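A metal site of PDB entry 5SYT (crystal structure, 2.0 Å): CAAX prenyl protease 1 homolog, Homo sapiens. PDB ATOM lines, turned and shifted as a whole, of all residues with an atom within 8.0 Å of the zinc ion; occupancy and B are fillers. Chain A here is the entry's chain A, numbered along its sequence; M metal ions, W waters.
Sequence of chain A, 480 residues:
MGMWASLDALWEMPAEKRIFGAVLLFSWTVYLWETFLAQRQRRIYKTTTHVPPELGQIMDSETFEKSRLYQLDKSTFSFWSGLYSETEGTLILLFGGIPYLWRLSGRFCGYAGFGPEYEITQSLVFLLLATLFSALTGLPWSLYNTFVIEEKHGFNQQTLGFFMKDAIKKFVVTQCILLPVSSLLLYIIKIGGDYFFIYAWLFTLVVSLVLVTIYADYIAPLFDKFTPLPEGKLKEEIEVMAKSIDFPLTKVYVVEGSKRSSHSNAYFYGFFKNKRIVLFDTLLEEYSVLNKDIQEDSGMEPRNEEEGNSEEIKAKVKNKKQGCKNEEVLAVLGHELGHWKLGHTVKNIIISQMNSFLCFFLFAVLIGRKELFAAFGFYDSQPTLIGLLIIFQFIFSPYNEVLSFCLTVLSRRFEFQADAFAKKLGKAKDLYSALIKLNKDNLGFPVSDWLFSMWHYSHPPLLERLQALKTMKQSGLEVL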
ATOM      1  N   VAL A 332      33.138 -23.030 -22.392  1.00  0.00           N
ATOM      2  CA  VAL A 332      33.147 -23.438 -21.000  1.00  0.00           C
ATOM      3  C   VAL A 332      33.788 -22.358 -20.150  1.00  0.00           C
ATOM      4  O   VAL A 332      33.305 -22.011 -19.064  1.00  0.00           O
ATOM      5  CB  VAL A 332      33.890 -24.776 -20.907  1.00  0.00           C
ATOM      6  CG1 VAL A 332      34.251 -25.137 -19.506  1.00  0.00           C
ATOM      7  CG2 VAL A 332      33.034 -25.885 -21.541  1.00  0.00           C
ATOM      8  N   HIS A 335      31.248 -19.694 -19.801  1.00  0.00           N
ATOM      9  CA  HIS A 335      30.382 -20.029 -18.675  1.00  0.00           C
ATOM     10  C   HIS A 335      31.038 -19.700 -17.350  1.00  0.00           C
ATOM     11  O   HIS A 335      30.451 -19.008 -16.497  1.00  0.00           O
ATOM     12  CB  HIS A 335      30.042 -21.524 -18.753  1.00  0.00           C
ATOM     13  CG  HIS A 335      29.446 -22.081 -17.511  1.00  0.00           C
ATOM     14  ND1 HIS A 335      28.102 -22.373 -17.412  1.00  0.00           N
ATOM     15  CD2 HIS A 335      29.998 -22.419 -16.325  1.00  0.00           C
ATOM     16  CE1 HIS A 335      27.852 -22.840 -16.200  1.00  0.00           C
ATOM     17  NE2 HIS A 335      28.981 -22.876 -15.522  1.00  0.00           N
ATOM     18  N   GLU A 336      32.245 -20.203 -17.117  1.00  0.00           N
ATOM     19  CA  GLU A 336      32.910 -19.933 -15.859  1.00  0.00           C
ATOM     20  C   GLU A 336      33.007 -18.432 -15.589  1.00  0.00           C
ATOM     21  O   GLU A 336      32.702 -17.972 -14.487  1.00  0.00           O
ATOM     22  CB  GLU A 336      34.283 -20.599 -15.849  1.00  0.00           C
ATOM     23  CG  GLU A 336      34.178 -22.106 -15.765  1.00  0.00           C
ATOM     24  CD  GLU A 336      33.303 -22.550 -14.572  1.00  0.00           C
ATOM     25  OE1 GLU A 336      33.359 -21.882 -13.502  1.00  0.00           O
ATOM     26  OE2 GLU A 336      32.531 -23.534 -14.730  1.00  0.00           O
ATOM     27  N   LEU A 337      33.431 -17.655 -16.591  1.00  0.00           N
ATOM     28  CA  LEU A 337      33.488 -16.211 -16.435  1.00  0.00           C
ATOM     29  C   LEU A 337      32.132 -15.599 -16.193  1.00  0.00           C
ATOM     30  O   LEU A 337      32.062 -14.490 -15.634  1.00  0.00           O
ATOM     31  CB  LEU A 337      34.091 -15.569 -17.681  1.00  0.00           C
ATOM     32  CG  LEU A 337      35.605 -15.715 -17.888  1.00  0.00           C
ATOM     33  CD1 LEU A 337      35.974 -15.386 -19.355  1.00  0.00           C
ATOM     34  CD2 LEU A 337      36.389 -14.832 -16.928  1.00  0.00           C
ATOM     35  N   GLY A 338      31.057 -16.255 -16.587  1.00  0.00           N
ATOM     36  CA  GLY A 338      29.735 -15.787 -16.191  1.00  0.00           C
ATOM     37  C   GLY A 338      29.531 -15.786 -14.691  1.00  0.00           C
ATOM     38  O   GLY A 338      28.858 -14.906 -14.143  1.00  0.00           O
ATOM     39  N   HIS A 339      30.113 -16.757 -13.983  1.00  0.00           N
ATOM     40  CA  HIS A 339      30.005 -16.745 -12.529  1.00  0.00           C
ATOM     41  C   HIS A 339      30.665 -15.500 -11.956  1.00  0.00           C
ATOM     42  O   HIS A 339      30.278 -15.012 -10.897  1.00  0.00           O
ATOM     43  CB  HIS A 339      30.656 -18.007 -11.959  1.00  0.00           C
ATOM     44  CG  HIS A 339      29.908 -19.283 -12.231  1.00  0.00           C
ATOM     45  ND1 HIS A 339      28.552 -19.409 -12.074  1.00  0.00           N
ATOM     46  CD2 HIS A 339      30.360 -20.511 -12.577  1.00  0.00           C
ATOM     47  CE1 HIS A 339      28.190 -20.653 -12.331  1.00  0.00           C
ATOM     48  NE2 HIS A 339      29.275 -21.353 -12.625  1.00  0.00           N
ATOM     49  N   HIS A 344      28.097 -14.184  -8.946  1.00  0.00           N
ATOM     50  CA  HIS A 344      27.690 -15.377  -8.205  1.00  0.00           C
ATOM     51  C   HIS A 344      28.674 -15.695  -7.100  1.00  0.00           C
ATOM     52  O   HIS A 344      28.279 -16.146  -6.006  1.00  0.00           O
ATOM     53  CB  HIS A 344      27.580 -16.596  -9.128  1.00  0.00           C
ATOM     54  CG  HIS A 344      26.515 -16.497 -10.154  1.00  0.00           C
ATOM     55  ND1 HIS A 344      26.541 -17.232 -11.317  1.00  0.00           N
ATOM     56  CD2 HIS A 344      25.389 -15.750 -10.203  1.00  0.00           C
ATOM     57  CE1 HIS A 344      25.472 -16.961 -12.044  1.00  0.00           C
ATOM     58  NE2 HIS A 344      24.761 -16.050 -11.393  1.00  0.00           N
ATOM     59  N   SER A 411      22.256 -22.897  -6.648  1.00  0.00           N
ATOM     60  CA  SER A 411      23.312 -23.353  -7.517  1.00  0.00           C
ATOM     61  C   SER A 411      22.801 -23.698  -8.922  1.00  0.00           C
ATOM     62  O   SER A 411      23.383 -23.298  -9.929  1.00  0.00           O
ATOM     63  CB  SER A 411      23.990 -24.547  -6.860  1.00  0.00           C
ATOM     64  OG  SER A 411      24.908 -25.175  -7.687  1.00  0.00           O
ATOM     65  N   PHE A 414      22.134 -20.506 -10.719  1.00  0.00           N
ATOM     66  CA  PHE A 414      23.359 -19.858 -11.185  1.00  0.00           C
ATOM     67  C   PHE A 414      23.930 -20.550 -12.406  1.00  0.00           C
ATOM     68  O   PHE A 414      24.491 -19.899 -13.302  1.00  0.00           O
ATOM     69  CB  PHE A 414      24.387 -19.836 -10.052  1.00  0.00           C
ATOM     70  CG  PHE A 414      24.109 -18.815  -8.989  1.00  0.00           C
ATOM     71  CD1 PHE A 414      23.064 -17.928  -9.114  1.00  0.00           C
ATOM     72  CD2 PHE A 414      24.912 -18.764  -7.863  1.00  0.00           C
ATOM     73  CE1 PHE A 414      22.821 -16.988  -8.141  1.00  0.00           C
ATOM     74  CE2 PHE A 414      24.688 -17.813  -6.883  1.00  0.00           C
ATOM     75  CZ  PHE A 414      23.643 -16.926  -7.009  1.00  0.00           C
ATOM     76  N   GLU A 415      23.820 -21.871 -12.454  1.00  0.00           N
ATOM     77  CA  GLU A 415      24.340 -22.586 -13.617  1.00  0.00           C
ATOM     78  C   GLU A 415      23.576 -22.217 -14.882  1.00  0.00           C
ATOM     79  O   GLU A 415      24.188 -22.010 -15.935  1.00  0.00           O
ATOM     80  CB  GLU A 415      24.300 -24.082 -13.351  1.00  0.00           C
ATOM     81  CG  GLU A 415      25.444 -24.506 -12.437  1.00  0.00           C
ATOM     82  CD  GLU A 415      26.779 -24.390 -13.119  1.00  0.00           C
ATOM     83  OE1 GLU A 415      27.142 -25.259 -13.932  1.00  0.00           O
ATOM     84  OE2 GLU A 415      27.476 -23.409 -12.851  1.00  0.00           O
ATOM     85  N   PHE A 416      22.252 -22.136 -14.816  1.00  0.00           N
ATOM     86  CA  PHE A 416      21.509 -21.719 -16.001  1.00  0.00           C
ATOM     87  C   PHE A 416      21.900 -20.305 -16.411  1.00  0.00           C
ATOM     88  O   PHE A 416      21.915 -19.968 -17.602  1.00  0.00           O
ATOM     89  CB  PHE A 416      20.000 -21.784 -15.740  1.00  0.00           C
ATOM     90  CG  PHE A 416      19.387 -23.144 -15.903  1.00  0.00           C
ATOM     91  CD1 PHE A 416      19.364 -23.774 -17.143  1.00  0.00           C
ATOM     92  CD2 PHE A 416      18.815 -23.786 -14.822  1.00  0.00           C
ATOM     93  CE1 PHE A 416      18.800 -25.020 -17.297  1.00  0.00           C
ATOM     94  CE2 PHE A 416      18.244 -25.052 -14.969  1.00  0.00           C
ATOM     95  CZ  PHE A 416      18.233 -25.667 -16.209  1.00  0.00           C
ATOM     96  N   GLN A 417      22.190 -19.454 -15.431  1.00  0.00           N
ATOM     97  CA  GLN A 417      22.563 -18.077 -15.714  1.00  0.00           C
ATOM     98  C   GLN A 417      23.946 -17.987 -16.350  1.00  0.00           C
ATOM     99  O   GLN A 417      24.178 -17.155 -17.232  1.00  0.00           O
ATOM    100  CB  GLN A 417      22.532 -17.273 -14.420  1.00  0.00           C
ATOM    101  CG  GLN A 417      21.154 -16.862 -14.030  1.00  0.00           C
ATOM    102  CD  GLN A 417      21.181 -16.158 -12.709  1.00  0.00           C
ATOM    103  OE1 GLN A 417      22.247 -15.766 -12.255  1.00  0.00           O
ATOM    104  NE2 GLN A 417      20.036 -16.004 -12.089  1.00  0.00           N
ATOM    105  N   ALA A 418      24.872 -18.802 -15.882  1.00  0.00           N
ATOM    106  CA  ALA A 418      26.183 -18.833 -16.498  1.00  0.00           C
ATOM    107  C   ALA A 418      26.108 -19.382 -17.923  1.00  0.00           C
ATOM    108  O   ALA A 418      26.698 -18.793 -18.844  1.00  0.00           O
ATOM    109  CB  ALA A 418      27.120 -19.631 -15.596  1.00  0.00           C
ATOM    110  N   ASP A 419      25.382 -20.481 -18.159  1.00  0.00           N
ATOM    111  CA  ASP A 419      25.114 -20.935 -19.526  1.00  0.00           C
ATOM    112  C   ASP A 419      24.587 -19.802 -20.393  1.00  0.00           C
ATOM    113  O   ASP A 419      25.012 -19.622 -21.529  1.00  0.00           O
ATOM    114  CB  ASP A 419      24.096 -22.092 -19.529  1.00  0.00           C
ATOM    115  CG  ASP A 419      24.689 -23.423 -19.065  1.00  0.00           C
ATOM    116  OD1 ASP A 419      25.910 -23.522 -18.885  1.00  0.00           O
ATOM    117  OD2 ASP A 419      23.907 -24.398 -18.917  1.00  0.00           O
ATOM    118  N   SER A 458      23.488 -30.148  -8.015  1.00  0.00           N
ATOM    119  CA  SER A 458      23.865 -28.735  -7.999  1.00  0.00           C
ATOM    120  C   SER A 458      23.983 -28.160  -9.397  1.00  0.00           C
ATOM    121  O   SER A 458      23.989 -26.933  -9.539  1.00  0.00           O
ATOM    122  CB  SER A 458      25.208 -28.545  -7.316  1.00  0.00           C
ATOM    123  OG  SER A 458      26.170 -29.287  -8.052  1.00  0.00           O
ATOM    124  N   HIS A 459      24.103 -29.011 -10.408  1.00  0.00           N
ATOM    125  CA  HIS A 459      24.022 -28.634 -11.804  1.00  0.00           C
ATOM    126  C   HIS A 459      22.765 -29.232 -12.390  1.00  0.00           C
ATOM    127  O   HIS A 459      22.476 -30.405 -12.124  1.00  0.00           O
ATOM    128  CB  HIS A 459      25.237 -29.144 -12.579  1.00  0.00           C
ATOM    129  CG  HIS A 459      26.537 -28.544 -12.136  1.00  0.00           C
ATOM    130  ND1 HIS A 459      27.319 -27.776 -12.975  1.00  0.00           N
ATOM    131  CD2 HIS A 459      27.211 -28.632 -10.967  1.00  0.00           C
ATOM    132  CE1 HIS A 459      28.406 -27.401 -12.340  1.00  0.00           C
ATOM    133  NE2 HIS A 459      28.369 -27.901 -11.113  1.00  0.00           N
ATOM    134  N   PRO A 460      21.990 -28.476 -13.175  1.00  0.00           N
ATOM    135  CA  PRO A 460      20.781 -29.061 -13.750  1.00  0.00           C
ATOM    136  C   PRO A 460      21.117 -30.143 -14.742  1.00  0.00           C
ATOM    137  O   PRO A 460      22.176 -30.109 -15.390  1.00  0.00           O
ATOM    138  CB  PRO A 460      20.096 -27.862 -14.427  1.00  0.00           C
ATOM    139  CG  PRO A 460      21.049 -26.704 -14.350  1.00  0.00           C
ATOM    140  CD  PRO A 460      22.211 -27.065 -13.512  1.00  0.00           C
ATOM    141  N   ARG A 465      19.982 -28.356 -19.684  1.00  0.00           N
ATOM    142  CA  ARG A 465      20.945 -27.335 -20.053  1.00  0.00           C
ATOM    143  C   ARG A 465      21.014 -27.174 -21.574  1.00  0.00           C
ATOM    144  O   ARG A 465      21.052 -26.064 -22.091  1.00  0.00           O
ATOM    145  CB  ARG A 465      22.312 -27.697 -19.461  1.00  0.00           C
ATOM    146  CG  ARG A 465      22.337 -27.730 -17.961  1.00  0.00           C
ATOM    147  CD  ARG A 465      23.675 -28.093 -17.374  1.00  0.00           C
ATOM    148  NE  ARG A 465      24.633 -27.004 -17.613  1.00  0.00           N
ATOM    149  CZ  ARG A 465      25.926 -27.020 -17.312  1.00  0.00           C
ATOM    150  NH1 ARG A 465      26.469 -28.089 -16.734  1.00  0.00           N
ATOM    151  NH2 ARG A 465      26.668 -25.974 -17.604  1.00  0.00           N
HETATM  152 ZN    ZN M   1      29.108 -23.160 -13.501  1.00  0.00          ZN
HETATM  153  O   HOH W   1      30.712 -24.197 -13.053  1.00  0.00           O
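The side-chain carboxylate (OE1) of Glu 415 is in hydrogen-bond range of a ring nitrogen (ND1) of His 459. OE1 of Glu 415 is in salt-bridge range of NH2 of Arg 465 (3.8 Å). The backbone carbonyl oxygen (O) of His 339 lies within hydrogen-bond range of the backbone NH (N) of His 344 (3.0 Å). The side-chain carboxylate (OD1) of Asp 419 lies within hydrogen-bond range of a ring nitrogen (ND1) of His 335 (2.9 Å).
Merely in contact with the zinc ion: Glu 336. Of the 18 residues printed, 4 come within 4 Å of the zinc ion. The nearest printed residue that does not touch the zinc ion is His 459 (4.5 Å).
The zinc ion is bound by OE2 of Glu 415 (1.8 Å), water W1 (2.0 Å), NE2 of His 339 (2.0 Å) and NE2 of His 335 (2.0 Å). The zinc ion has four donor atoms within binding distance.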
